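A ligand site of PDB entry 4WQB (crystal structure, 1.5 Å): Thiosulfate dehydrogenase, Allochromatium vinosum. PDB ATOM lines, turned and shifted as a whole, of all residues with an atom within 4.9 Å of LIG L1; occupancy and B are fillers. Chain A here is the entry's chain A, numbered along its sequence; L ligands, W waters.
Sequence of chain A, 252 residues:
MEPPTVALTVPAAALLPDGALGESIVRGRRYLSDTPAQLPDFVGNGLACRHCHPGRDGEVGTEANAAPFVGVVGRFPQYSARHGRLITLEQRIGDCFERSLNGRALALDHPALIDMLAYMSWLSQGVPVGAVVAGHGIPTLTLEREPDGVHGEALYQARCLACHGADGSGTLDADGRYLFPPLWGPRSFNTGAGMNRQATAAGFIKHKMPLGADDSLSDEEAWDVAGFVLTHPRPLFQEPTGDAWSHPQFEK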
ATOM      1  N   LEU A  32      31.027  -0.480 -18.016  1.00  0.00           N
ATOM      2  CA  LEU A  32      31.119   0.574 -17.005  1.00  0.00           C
ATOM      3  C   LEU A  32      32.537   0.683 -16.434  1.00  0.00           C
ATOM      4  O   LEU A  32      32.956   1.744 -16.033  1.00  0.00           O
ATOM      5  CB  LEU A  32      30.116   0.305 -15.900  1.00  0.00           C
ATOM      6  CG  LEU A  32      28.646   0.391 -16.334  1.00  0.00           C
ATOM      7  CD1 LEU A  32      27.747  -0.227 -15.267  1.00  0.00           C
ATOM      8  CD2 LEU A  32      28.248   1.842 -16.565  1.00  0.00           C
ATOM      9  N   THR A  35      35.332   1.545 -20.111  1.00  0.00           N
ATOM     10  CA  THR A  35      34.509   2.134 -21.162  1.00  0.00           C
ATOM     11  C   THR A  35      35.288   2.582 -22.400  1.00  0.00           C
ATOM     12  O   THR A  35      34.855   2.276 -23.513  1.00  0.00           O
ATOM     13  CB  THR A  35      33.721   3.325 -20.610  1.00  0.00           C
ATOM     14  OG1 THR A  35      33.416   3.089 -19.228  1.00  0.00           O
ATOM     15  CG2 THR A  35      32.444   3.485 -21.389  1.00  0.00           C
ATOM     16  N   LEU A  47      38.375   8.537 -19.653  1.00  0.00           N
ATOM     17  CA  LEU A  47      37.640   8.141 -18.454  1.00  0.00           C
ATOM     18  C   LEU A  47      36.695   6.965 -18.701  1.00  0.00           C
ATOM     19  O   LEU A  47      36.056   6.831 -19.755  1.00  0.00           O
ATOM     20  CB  LEU A  47      36.858   9.328 -17.881  1.00  0.00           C
ATOM     21  CG  LEU A  47      37.687  10.541 -17.473  1.00  0.00           C
ATOM     22  CD1 LEU A  47      36.814  11.568 -16.850  1.00  0.00           C
ATOM     23  CD2 LEU A  47      38.845  10.150 -16.565  1.00  0.00           C
ATOM     24  N   ALA A  48      36.661   6.089 -17.707  1.00  0.00           N
ATOM     25  CA  ALA A  48      35.640   5.060 -17.591  1.00  0.00           C
ATOM     26  C   ALA A  48      34.627   5.509 -16.559  1.00  0.00           C
ATOM     27  O   ALA A  48      34.917   6.322 -15.706  1.00  0.00           O
ATOM     28  CB  ALA A  48      36.243   3.727 -17.200  1.00  0.00           C
ATOM     29  N   CYS A  49      33.427   4.955 -16.613  1.00  0.00           N
ATOM     30  CA  CYS A  49      32.398   5.346 -15.655  1.00  0.00           C
ATOM     31  C   CYS A  49      32.914   5.155 -14.216  1.00  0.00           C
ATOM     32  O   CYS A  49      32.611   5.952 -13.348  1.00  0.00           O
ATOM     33  CB  CYS A  49      31.109   4.544 -15.879  1.00  0.00           C
ATOM     34  SG  CYS A  49      30.538   4.501 -17.594  1.00  0.00           S
ATOM     35  N   CYS A  52      34.521   7.935 -11.616  1.00  0.00           N
ATOM     36  CA  CYS A  52      33.746   8.778 -10.713  1.00  0.00           C
ATOM     37  C   CYS A  52      32.675   7.998  -9.963  1.00  0.00           C
ATOM     38  O   CYS A  52      32.097   8.498  -9.006  1.00  0.00           O
ATOM     39  CB  CYS A  52      33.078   9.919 -11.454  1.00  0.00           C
ATOM     40  SG  CYS A  52      34.264  10.996 -12.270  1.00  0.00           S
ATOM     41  N   HIS A  53      32.431   6.767 -10.419  1.00  0.00           N
ATOM     42  CA  HIS A  53      31.444   5.879  -9.826  1.00  0.00           C
ATOM     43  C   HIS A  53      32.148   4.592  -9.370  1.00  0.00           C
ATOM     44  O   HIS A  53      31.913   3.505  -9.917  1.00  0.00           O
ATOM     45  CB  HIS A  53      30.340   5.525 -10.832  1.00  0.00           C
ATOM     46  CG  HIS A  53      29.550   6.702 -11.339  1.00  0.00           C
ATOM     47  ND1 HIS A  53      28.472   7.210 -10.652  1.00  0.00           N
ATOM     48  CD2 HIS A  53      29.642   7.419 -12.480  1.00  0.00           C
ATOM     49  CE1 HIS A  53      27.939   8.206 -11.339  1.00  0.00           C
ATOM     50  NE2 HIS A  53      28.630   8.357 -12.453  1.00  0.00           N
ATOM     51  N   ALA A  67      28.075   8.543  -6.012  1.00  0.00           N
ATOM     52  CA  ALA A  67      27.016   8.340  -6.994  1.00  0.00           C
ATOM     53  C   ALA A  67      26.822   6.851  -7.319  1.00  0.00           C
ATOM     54  O   ALA A  67      26.932   6.439  -8.463  1.00  0.00           O
ATOM     55  CB  ALA A  67      27.300   9.133  -8.256  1.00  0.00           C
ATOM     56  N   PRO A  68      26.533   6.052  -6.305  1.00  0.00           N
ATOM     57  CA  PRO A  68      26.296   4.635  -6.583  1.00  0.00           C
ATOM     58  C   PRO A  68      25.111   4.421  -7.507  1.00  0.00           C
ATOM     59  O   PRO A  68      24.166   5.234  -7.550  1.00  0.00           O
ATOM     60  CB  PRO A  68      26.012   4.051  -5.191  1.00  0.00           C
ATOM     61  CG  PRO A  68      25.470   5.205  -4.425  1.00  0.00           C
ATOM     62  CD  PRO A  68      26.218   6.403  -4.910  1.00  0.00           C
ATOM     63  N   PHE A  69      25.152   3.321  -8.252  1.00  0.00           N
ATOM     64  CA  PHE A  69      24.053   2.942  -9.127  1.00  0.00           C
ATOM     65  C   PHE A  69      23.051   2.039  -8.414  1.00  0.00           C
ATOM     66  O   PHE A  69      21.999   1.689  -8.973  1.00  0.00           O
ATOM     67  CB  PHE A  69      24.585   2.223 -10.364  1.00  0.00           C
ATOM     68  CG  PHE A  69      25.507   3.041 -11.214  1.00  0.00           C
ATOM     69  CD1 PHE A  69      25.284   4.396 -11.422  1.00  0.00           C
ATOM     70  CD2 PHE A  69      26.593   2.442 -11.833  1.00  0.00           C
ATOM     71  CE1 PHE A  69      26.136   5.120 -12.219  1.00  0.00           C
ATOM     72  CE2 PHE A  69      27.434   3.161 -12.623  1.00  0.00           C
ATOM     73  CZ  PHE A  69      27.231   4.507 -12.820  1.00  0.00           C
ATOM     74  N   VAL A  72      19.399   3.208  -8.616  1.00  0.00           N
ATOM     75  CA  VAL A  72      19.208   4.305  -9.550  1.00  0.00           C
ATOM     76  C   VAL A  72      18.018   4.057 -10.474  1.00  0.00           C
ATOM     77  O   VAL A  72      17.332   4.992 -10.868  1.00  0.00           O
ATOM     78  CB  VAL A  72      20.497   4.578 -10.367  1.00  0.00           C
ATOM     79  CG1 VAL A  72      20.753   3.480 -11.370  1.00  0.00           C
ATOM     80  CG2 VAL A  72      20.417   5.939 -11.058  1.00  0.00           C
ATOM     81  N   PHE A  76      14.134   6.848 -12.047  1.00  0.00           N
ATOM     82  CA  PHE A  76      13.847   7.345 -13.380  1.00  0.00           C
ATOM     83  C   PHE A  76      12.539   6.717 -13.903  1.00  0.00           C
ATOM     84  O   PHE A  76      12.211   5.589 -13.532  1.00  0.00           O
ATOM     85  CB  PHE A  76      14.991   7.009 -14.331  1.00  0.00           C
ATOM     86  CG  PHE A  76      16.197   7.867 -14.105  1.00  0.00           C
ATOM     87  CD1 PHE A  76      17.102   7.566 -13.109  1.00  0.00           C
ATOM     88  CD2 PHE A  76      16.433   8.993 -14.887  1.00  0.00           C
ATOM     89  CE1 PHE A  76      18.216   8.362 -12.887  1.00  0.00           C
ATOM     90  CE2 PHE A  76      17.531   9.804 -14.654  1.00  0.00           C
ATOM     91  CZ  PHE A  76      18.422   9.468 -13.660  1.00  0.00           C
ATOM     92  N   GLN A  78      12.674  10.995 -14.505  1.00  0.00           N
ATOM     93  CA  GLN A  78      12.685  12.111 -13.586  1.00  0.00           C
ATOM     94  C   GLN A  78      12.916  13.393 -14.362  1.00  0.00           C
ATOM     95  O   GLN A  78      13.426  13.378 -15.477  1.00  0.00           O
ATOM     96  CB  GLN A  78      13.787  11.933 -12.536  1.00  0.00           C
ATOM     97  CG  GLN A  78      15.169  12.055 -13.117  1.00  0.00           C
ATOM     98  CD  GLN A  78      16.301  11.773 -12.126  1.00  0.00           C
ATOM     99  OE1 GLN A  78      16.206  10.900 -11.227  1.00  0.00           O
ATOM    100  NE2 GLN A  78      17.371  12.487 -12.290  1.00  0.00           N
ATOM    101  N   LEU A  89      16.492   6.890 -17.778  1.00  0.00           N
ATOM    102  CA  LEU A  89      17.847   6.512 -17.416  1.00  0.00           C
ATOM    103  C   LEU A  89      18.748   6.349 -18.644  1.00  0.00           C
ATOM    104  O   LEU A  89      19.926   6.707 -18.592  1.00  0.00           O
ATOM    105  CB  LEU A  89      17.841   5.232 -16.587  1.00  0.00           C
ATOM    106  CG  LEU A  89      19.178   4.683 -16.079  1.00  0.00           C
ATOM    107  CD1 LEU A  89      19.989   5.740 -15.352  1.00  0.00           C
ATOM    108  CD2 LEU A  89      18.933   3.525 -15.149  1.00  0.00           C
ATOM    109  N   ARG A  92      19.893   9.756 -19.443  1.00  0.00           N
ATOM    110  CA  ARG A  92      20.858  10.208 -18.442  1.00  0.00           C
ATOM    111  C   ARG A  92      22.236   9.633 -18.766  1.00  0.00           C
ATOM    112  O   ARG A  92      23.230  10.352 -18.740  1.00  0.00           O
ATOM    113  CB  ARG A  92      20.413   9.777 -17.042  1.00  0.00           C
ATOM    114  CG  ARG A  92      21.331  10.192 -15.901  1.00  0.00           C
ATOM    115  CD  ARG A  92      21.125  11.676 -15.640  1.00  0.00           C
ATOM    116  NE  ARG A  92      22.038  12.241 -14.666  1.00  0.00           N
ATOM    117  CZ  ARG A  92      23.269  12.644 -14.963  1.00  0.00           C
ATOM    118  NH1 ARG A  92      23.743  12.493 -16.191  1.00  0.00           N
ATOM    119  NH2 ARG A  92      24.037  13.200 -14.029  1.00  0.00           N
ATOM    120  N   ILE A  93      22.279   8.341 -19.082  1.00  0.00           N
ATOM    121  CA  ILE A  93      23.557   7.722 -19.438  1.00  0.00           C
ATOM    122  C   ILE A  93      24.168   8.377 -20.673  1.00  0.00           C
ATOM    123  O   ILE A  93      25.374   8.593 -20.736  1.00  0.00           O
ATOM    124  CB  ILE A  93      23.381   6.202 -19.642  1.00  0.00           C
ATOM    125  CG1 ILE A  93      23.069   5.565 -18.272  1.00  0.00           C
ATOM    126  CG2 ILE A  93      24.621   5.564 -20.267  1.00  0.00           C
ATOM    127  CD1 ILE A  93      22.604   4.115 -18.305  1.00  0.00           C
ATOM    128  N   CSS A  96      25.963  11.463 -19.762  1.00  0.00           N
ATOM    129  CA  CSS A  96      27.249  11.137 -19.183  1.00  0.00           C
ATOM    130  CB  CSS A  96      27.140   9.962 -18.201  1.00  0.00           C
ATOM    131  SG  CSS A  96      26.068  10.321 -16.857  1.00  0.00           S
ATOM    132  SD  CSS A  96      27.463  11.192 -15.571  1.00  0.00           S
ATOM    133  C   CSS A  96      28.306  10.841 -20.233  1.00  0.00           C
ATOM    134  O   CSS A  96      29.459  11.237 -20.142  1.00  0.00           O
ATOM    135  N   PHE A  97      27.916  10.091 -21.277  1.00  0.00           N
ATOM    136  CA  PHE A  97      28.832   9.843 -22.380  1.00  0.00           C
ATOM    137  C   PHE A  97      29.254  11.148 -23.050  1.00  0.00           C
ATOM    138  O   PHE A  97      30.429  11.332 -23.363  1.00  0.00           O
ATOM    139  CB  PHE A  97      28.212   8.906 -23.429  1.00  0.00           C
ATOM    140  CG  PHE A  97      28.480   7.438 -23.163  1.00  0.00           C
ATOM    141  CD1 PHE A  97      27.621   6.704 -22.371  1.00  0.00           C
ATOM    142  CD2 PHE A  97      29.588   6.815 -23.679  1.00  0.00           C
ATOM    143  CE1 PHE A  97      27.845   5.362 -22.136  1.00  0.00           C
ATOM    144  CE2 PHE A  97      29.822   5.476 -23.442  1.00  0.00           C
ATOM    145  CZ  PHE A  97      28.951   4.761 -22.657  1.00  0.00           C
ATOM    146  N   SER A 100      30.795  13.737 -19.277  1.00  0.00           N
ATOM    147  CA  SER A 100      31.873  13.147 -18.479  1.00  0.00           C
ATOM    148  C   SER A 100      32.882  12.382 -19.324  1.00  0.00           C
ATOM    149  O   SER A 100      34.081  12.380 -18.988  1.00  0.00           O
ATOM    150  CB  SER A 100      31.293  12.219 -17.420  1.00  0.00           C
ATOM    151  OG  SER A 100      30.521  12.964 -16.505  1.00  0.00           O
ATOM    152  N   LEU A 101      32.416  11.747 -20.387  1.00  0.00           N
ATOM    153  CA  LEU A 101      33.307  10.998 -21.271  1.00  0.00           C
ATOM    154  C   LEU A 101      33.582  11.693 -22.608  1.00  0.00           C
ATOM    155  O   LEU A 101      34.204  11.127 -23.483  1.00  0.00           O
ATOM    156  CB  LEU A 101      32.757   9.585 -21.499  1.00  0.00           C
ATOM    157  CG  LEU A 101      33.239   8.535 -20.508  1.00  0.00           C
ATOM    158  CD1 LEU A 101      33.017   8.883 -19.065  1.00  0.00           C
ATOM    159  CD2 LEU A 101      32.625   7.182 -20.814  1.00  0.00           C
ATOM    160  N   MET A 116      24.338  -2.129 -19.814  1.00  0.00           N
ATOM    161  CA  MET A 116      24.606  -1.235 -18.694  1.00  0.00           C
ATOM    162  C   MET A 116      23.362  -1.080 -17.819  1.00  0.00           C
ATOM    163  O   MET A 116      23.456  -1.102 -16.595  1.00  0.00           O
ATOM    164  CB  MET A 116      25.081   0.141 -19.194  1.00  0.00           C
ATOM    165  CG  MET A 116      26.492   0.090 -19.740  1.00  0.00           C
ATOM    166  SD  MET A 116      27.098   1.720 -20.210  1.00  0.00           S
ATOM    167  CE  MET A 116      26.759   1.757 -21.953  1.00  0.00           C
ATOM    168  N   MET A 120      22.887  -2.081 -13.847  1.00  0.00           N
ATOM    169  CA  MET A 120      22.346  -1.176 -12.829  1.00  0.00           C
ATOM    170  C   MET A 120      21.083  -1.743 -12.196  1.00  0.00           C
ATOM    171  O   MET A 120      20.853  -1.572 -11.002  1.00  0.00           O
ATOM    172  CB  MET A 120      22.069   0.193 -13.436  1.00  0.00           C
ATOM    173  CG  MET A 120      23.299   0.906 -13.933  1.00  0.00           C
ATOM    174  SD  MET A 120      22.882   2.523 -14.552  1.00  0.00           S
ATOM    175  CE  MET A 120      24.486   3.024 -15.176  1.00  0.00           C
ATOM    176  N   GLY A 137      24.056   9.553  -4.969  1.00  0.00           N
ATOM    177  CA  GLY A 137      24.573  10.792  -5.515  1.00  0.00           C
ATOM    178  C   GLY A 137      25.944  11.171  -4.963  1.00  0.00           C
ATOM    179  O   GLY A 137      26.609  10.368  -4.297  1.00  0.00           O
ATOM    180  N   ILE A 138      26.371  12.393  -5.287  1.00  0.00           N
ATOM    181  CA  ILE A 138      27.588  12.973  -4.742  1.00  0.00           C
ATOM    182  C   ILE A 138      27.137  14.223  -3.982  1.00  0.00           C
ATOM    183  O   ILE A 138      26.774  15.215  -4.596  1.00  0.00           O
ATOM    184  CB  ILE A 138      28.611  13.310  -5.843  1.00  0.00           C
ATOM    185  CG1 ILE A 138      29.148  12.016  -6.452  1.00  0.00           C
ATOM    186  CG2 ILE A 138      29.787  14.132  -5.282  1.00  0.00           C
ATOM    187  CD1 ILE A 138      29.807  12.180  -7.792  1.00  0.00           C
ATOM    188  N   PHE A 189      37.328  14.987 -18.155  1.00  0.00           N
ATOM    189  CA  PHE A 189      35.942  15.353 -18.420  1.00  0.00           C
ATOM    190  C   PHE A 189      35.855  16.738 -19.052  1.00  0.00           C
ATOM    191  O   PHE A 189      36.754  17.560 -18.862  1.00  0.00           O
ATOM    192  CB  PHE A 189      35.116  15.271 -17.128  1.00  0.00           C
ATOM    193  CG  PHE A 189      35.614  16.125 -15.990  1.00  0.00           C
ATOM    194  CD1 PHE A 189      35.224  17.458 -15.863  1.00  0.00           C
ATOM    195  CD2 PHE A 189      36.425  15.573 -15.004  1.00  0.00           C
ATOM    196  CE1 PHE A 189      35.661  18.212 -14.799  1.00  0.00           C
ATOM    197  CE2 PHE A 189      36.872  16.330 -13.938  1.00  0.00           C
ATOM    198  CZ  PHE A 189      36.487  17.659 -13.833  1.00  0.00           C
ATOM    199  N   GLY A 194      29.119  17.358 -14.712  1.00  0.00           N
ATOM    200  CA  GLY A 194      28.814  17.751 -13.344  1.00  0.00           C
ATOM    201  C   GLY A 194      30.064  17.963 -12.516  1.00  0.00           C
ATOM    202  O   GLY A 194      30.093  18.820 -11.643  1.00  0.00           O
ATOM    203  N   MET A 195      31.098  17.182 -12.787  1.00  0.00           N
ATOM    204  CA  MET A 195      32.348  17.298 -12.032  1.00  0.00           C
ATOM    205  C   MET A 195      33.070  18.636 -12.275  1.00  0.00           C
ATOM    206  O   MET A 195      33.973  18.997 -11.527  1.00  0.00           O
ATOM    207  CB  MET A 195      33.257  16.110 -12.348  1.00  0.00           C
ATOM    208  CG  MET A 195      34.369  15.922 -11.331  1.00  0.00           C
ATOM    209  SD  MET A 195      33.851  15.546  -9.649  1.00  0.00           S
ATOM    210  CE  MET A 195      33.273  13.864  -9.851  1.00  0.00           C
ATOM    211  N   THR A 200      30.247  20.278  -6.597  1.00  0.00           N
ATOM    212  CA  THR A 200      30.238  18.843  -6.861  1.00  0.00           C
ATOM    213  C   THR A 200      31.646  18.279  -6.739  1.00  0.00           C
ATOM    214  O   THR A 200      31.853  17.291  -6.034  1.00  0.00           O
ATOM    215  CB  THR A 200      29.647  18.556  -8.241  1.00  0.00           C
ATOM    216  OG1 THR A 200      28.264  18.937  -8.214  1.00  0.00           O
ATOM    217  CG2 THR A 200      29.747  17.097  -8.600  1.00  0.00           C
HETATM  218 FE1  LIG L   1      28.074   9.685 -13.934  1.00  0.00          FE
HETATM  219  C1  LIG L   1      25.399  10.984 -12.075  1.00  0.00           C
HETATM  220  C2  LIG L   1      25.994   7.138 -15.142  1.00  0.00           C
HETATM  221  C3  LIG L   1      30.633   8.563 -15.950  1.00  0.00           C
HETATM  222  C4  LIG L   1      30.221  12.081 -12.474  1.00  0.00           C
HETATM  223  N1  LIG L   1      26.093   9.163 -13.684  1.00  0.00           N
HETATM  224  C5  LIG L   1      25.209   9.788 -12.882  1.00  0.00           C
HETATM  225  C6  LIG L   1      23.888   9.155 -12.898  1.00  0.00           C
HETATM  226  C7  LIG L   1      24.064   8.009 -13.793  1.00  0.00           C
HETATM  227  C8  LIG L   1      25.462   8.110 -14.207  1.00  0.00           C
HETATM  228  C9  LIG L   1      23.071   6.972 -14.196  1.00  0.00           C
HETATM  229  C10 LIG L   1      22.661   9.553 -12.123  1.00  0.00           C
HETATM  230  C11 LIG L   1      22.827   9.012 -10.688  1.00  0.00           C
HETATM  231  C12 LIG L   1      21.627   9.295  -9.817  1.00  0.00           C
HETATM  232  O1  LIG L   1      21.660   8.908  -8.624  1.00  0.00           O
HETATM  233  O2  LIG L   1      20.644   9.897 -10.318  1.00  0.00           O
HETATM  234  N2  LIG L   1      28.256   8.156 -15.279  1.00  0.00           N
HETATM  235  C13 LIG L   1      27.336   7.247 -15.628  1.00  0.00           C
HETATM  236  C14 LIG L   1      27.806   6.313 -16.636  1.00  0.00           C
HETATM  237  C15 LIG L   1      29.180   6.723 -16.883  1.00  0.00           C
HETATM  238  C16 LIG L   1      29.333   7.899 -15.993  1.00  0.00           C
HETATM  239  C17 LIG L   1      27.070   5.172 -17.228  1.00  0.00           C
HETATM  240  C18 LIG L   1      30.142   6.133 -17.863  1.00  0.00           C
HETATM  241  C19 LIG L   1      29.538   6.230 -19.263  1.00  0.00           C
HETATM  242  N3  LIG L   1      30.036  10.243 -14.176  1.00  0.00           N
HETATM  243  C20 LIG L   1      30.892   9.641 -15.008  1.00  0.00           C
HETATM  244  C21 LIG L   1      32.259  10.186 -14.905  1.00  0.00           C
HETATM  245  C22 LIG L   1      32.133  11.236 -13.893  1.00  0.00           C
HETATM  246  C23 LIG L   1      30.720  11.177 -13.489  1.00  0.00           C
HETATM  247  C24 LIG L   1      33.473   9.744 -15.685  1.00  0.00           C
HETATM  248  C25 LIG L   1      33.204  12.129 -13.330  1.00  0.00           C
HETATM  249  C26 LIG L   1      34.003  12.876 -14.363  1.00  0.00           C
HETATM  250  N4  LIG L   1      27.866  11.201 -12.566  1.00  0.00           N
HETATM  251  C27 LIG L   1      28.815  12.046 -12.114  1.00  0.00           C
HETATM  252  C28 LIG L   1      28.286  13.061 -11.177  1.00  0.00           C
HETATM  253  C29 LIG L   1      26.884  12.755 -11.061  1.00  0.00           C
HETATM  254  C30 LIG L   1      26.731  11.592 -11.958  1.00  0.00           C
HETATM  255  C31 LIG L   1      29.053  14.144 -10.502  1.00  0.00           C
HETATM  256  C32 LIG L   1      25.854  13.451 -10.210  1.00  0.00           C
HETATM  257  C33 LIG L   1      25.550  12.655  -8.952  1.00  0.00           C
HETATM  258  C34 LIG L   1      24.392  13.282  -8.221  1.00  0.00           C
HETATM  259  O3  LIG L   1      23.293  13.343  -8.807  1.00  0.00           O
HETATM  260  O4  LIG L   1      24.564  13.732  -7.067  1.00  0.00           O
HETATM  261 FE1  LG2 L   2      41.937  11.132  -6.948  1.00  0.00          FE
HETATM  262  C1  LG2 L   2      39.342   9.864  -8.931  1.00  0.00           C
HETATM  263  C2  LG2 L   2      40.680  14.371  -7.345  1.00  0.00           C
HETATM  264  C3  LG2 L   2      44.203  12.299  -4.556  1.00  0.00           C
HETATM  265  C4  LG2 L   2      43.541   8.061  -7.040  1.00  0.00           C
HETATM  266  N1  LG2 L   2      40.336  11.970  -7.944  1.00  0.00           N
HETATM  267  C5  LG2 L   2      39.445  11.300  -8.713  1.00  0.00           C
HETATM  268  C6  LG2 L   2      38.466  12.203  -9.299  1.00  0.00           C
HETATM  269  C7  LG2 L   2      38.871  13.531  -8.836  1.00  0.00           C
HETATM  270  C8  LG2 L   2      40.025  13.263  -7.996  1.00  0.00           C
HETATM  271  C9  LG2 L   2      38.196  14.840  -9.120  1.00  0.00           C
HETATM  272  C10 LG2 L   2      37.337  11.869 -10.207  1.00  0.00           C
HETATM  273  C11 LG2 L   2      37.872  11.400 -11.578  1.00  0.00           C
HETATM  274  C12 LG2 L   2      38.510  12.432 -12.508  1.00  0.00           C
HETATM  275  O1  LG2 L   2      39.352  12.026 -13.366  1.00  0.00           O
HETATM  276  O2  LG2 L   2      38.237  13.637 -12.443  1.00  0.00           O
HETATM  277  N2  LG2 L   2      42.337  12.963  -6.125  1.00  0.00           N
HETATM  278  C13 LG2 L   2      41.755  14.133  -6.404  1.00  0.00           C
HETATM  279  C14 LG2 L   2      42.293  15.225  -5.598  1.00  0.00           C
HETATM  280  C15 LG2 L   2      43.295  14.609  -4.769  1.00  0.00           C
HETATM  281  C16 LG2 L   2      43.253  13.195  -5.171  1.00  0.00           C
HETATM  282  C17 LG2 L   2      41.929  16.666  -5.613  1.00  0.00           C
HETATM  283  C18 LG2 L   2      44.183  15.235  -3.727  1.00  0.00           C
HETATM  284  C19 LG2 L   2      43.266  15.709  -2.595  1.00  0.00           C
HETATM  285  N3  LG2 L   2      43.571  10.331  -5.987  1.00  0.00           N
HETATM  286  C20 LG2 L   2      44.348  10.928  -5.081  1.00  0.00           C
HETATM  287  C21 LG2 L   2      45.481  10.084  -4.661  1.00  0.00           C
HETATM  288  C22 LG2 L   2      45.311   8.849  -5.392  1.00  0.00           C
HETATM  289  C23 LG2 L   2      44.098   9.104  -6.193  1.00  0.00           C
HETATM  290  C24 LG2 L   2      46.567  10.427  -3.705  1.00  0.00           C
HETATM  291  C25 LG2 L   2      46.210   7.632  -5.421  1.00  0.00           C
HETATM  292  C26 LG2 L   2      46.416   6.917  -4.130  1.00  0.00           C
HETATM  293  N4  LG2 L   2      41.532   9.320  -7.808  1.00  0.00           N
HETATM  294  C27 LG2 L   2      42.264   8.204  -7.719  1.00  0.00           C
HETATM  295  C28 LG2 L   2      41.600   7.059  -8.394  1.00  0.00           C
HETATM  296  C29 LG2 L   2      40.382   7.607  -8.922  1.00  0.00           C
HETATM  297  C30 LG2 L   2      40.420   9.000  -8.485  1.00  0.00           C
HETATM  298  C31 LG2 L   2      42.084   5.663  -8.524  1.00  0.00           C
HETATM  299  C32 LG2 L   2      39.293   6.922  -9.679  1.00  0.00           C
HETATM  300  C33 LG2 L   2      38.103   6.725  -8.713  1.00  0.00           C
HETATM  301  C34 LG2 L   2      38.317   5.667  -7.635  1.00  0.00           C
HETATM  302  O3  LG2 L   2      38.088   5.991  -6.457  1.00  0.00           O
HETATM  303  O4  LG2 L   2      38.667   4.497  -7.920  1.00  0.00           O
HETATM  304  O   HOH W   1      19.979   7.237  -7.203  1.00  0.00           O
HETATM  305  O   HOH W   2      22.274  13.449 -11.334  1.00  0.00           O
HETATM  306  O   HOH W   3      18.336  10.588  -9.190  1.00  0.00           O
HETATM  307  O   HOH W   4      21.158  10.831  -6.659  1.00  0.00           O
HETATM  308  O   HOH W   5      22.855  14.508  -5.314  1.00  0.00           O
HETATM  309  O   HOH W   6      30.600  14.682 -14.222  1.00  0.00           O
HETATM  310  O   HOH W   7      26.618  16.475  -7.090  1.00  0.00           O
HETATM  311  O   HOH W   8      20.843  13.481  -7.593  1.00  0.00           O
HETATM  312  O   HOH W   9      23.710   7.891  -7.166  1.00  0.00           O
HETATM  313  O   HOH W  10      20.221  11.999 -12.040  1.00  0.00           O
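The backbone NH (N) of Ala 67 sits at hydrogen-bond distance from the backbone carbonyl oxygen (O) of Gly 137 (2.9 Å).
SG of CSS 96 lies within hydrogen-bond range of the guanidinium group (NH1) of Arg 92 (3.3 Å).
The backbone carbonyl oxygen (O) of Leu 32 is in hydrogen-bond range of the side-chain hydroxyl (OG1) of Thr 35.
The backbone NH (N) of Cys 49 sits at hydrogen-bond distance from the side-chain hydroxyl (OG1) of Thr 35, 3.2 Å away.
N of Cys 49 sits at hydrogen-bond distance from O of Leu 32.
SD of CSS 96 sits close to the side-chain hydroxyl of Ser 100 (3.7 Å).
N of Leu 101 sits at hydrogen-bond distance from O of CSS 96 (3.0 Å).
A ring nitrogen (ND1) of His 53 is in hydrogen-bond range of the backbone carbonyl oxygen of Ala 67 (2.8 Å).
Water W3 lies within hydrogen-bond range of O2 of LIG L1 (2.7 Å) and OE1 of Gln 78 (3.0 Å).
Water W9 lies within hydrogen-bond range of O1 of LIG L1 (2.7 Å), O of Pro 68 (2.7 Å) and N of Gly 137 (2.8 Å).
Water W2 lies within hydrogen-bond range of an oxygen (O3) of LIG L1 (2.7 Å) and the guanidinium group (NH2) of Arg 92 (3.2 Å).
Water W10 lies within hydrogen-bond range of O2 of LIG L1 (2.8 Å), NE2 of Gln 78 (2.9 Å) and NE of Arg 92 (3.2 Å).
Water W6 lies within hydrogen-bond range of the side-chain hydroxyl of Ser 100, the backbone NH of Met 195 and the backbone NH of Gly 194.
Water W7 lies within hydrogen-bond range of the backbone carbonyl oxygen (O) of Ile 138 (2.8 Å), the side-chain hydroxyl (OG1) of Thr 200 (3.2 Å) and an oxygen (O4) of LIG L1 (3.4 Å).
The side-chain sulfur of Cys 49 is bonded to a carbon (C18) of LIG L1, at 1.7 Å.
NE2 of His 53 binds FE1 of LIG L1, at 2.1 Å.
The side-chain sulfur (SG) of Cys 52 is bonded to a carbon (C25) of LIG L1 (1.9 Å).
The backbone NH of Ile 138 sits at hydrogen-bond distance from an oxygen (O4) of LIG L1, at 2.9 Å.
SD of CSS 96 binds an iron atom (FE1) of LIG L1 (2.3 Å).
Leu 32 touches LIG L1.
CD1 of Leu 47 touches C26 of LIG L1 (3.97 Å).
Ala 48 touches LIG L1 (O to C24, 3.7 Å).
CB of Ala 67 touches C33 of LIG L1, at 3.99 Å.
Phe 69 touches LIG L1.
Val 72 touches LIG L1.
Phe 76 touches LIG L1 (CE1 to O2, 3.9 Å).
CD1 of Leu 89 touches C9 of LIG L1 (3.5 Å).
Arg 92 touches LIG L1 (NH2 to C1, 3.3 Å).
Ile 93 touches LIG L1 (CG2 to C17, 3.9 Å).
CE1 of Phe 97 touches C19 of LIG L1 (3.4 Å).
Ser 100 touches LIG L1 (CB to C21, 3.4 Å).
Leu 101 touches LIG L1.
Met 120 touches LIG L1.
Gly 137 touches LIG L1 (CA to O4, 3.3 Å).
Phe 189 touches LIG L1.
Met 195 touches LIG L1 (CB to C26, 3.9 Å).
Thr 200 touches LIG L1.
Hydrophobic or aromatic side chains that line LIG L1: Leu 32, Leu 47, His 53, Ala 67, Phe 69, Val 72, Phe 76, Leu 89, Ile 93, Phe 97, Leu 101, Met 120, Ile 138, Phe 189 and Met 195.
The nearest printed residue that does not touch LIG L1 is Gly 194 (4.4 Å).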
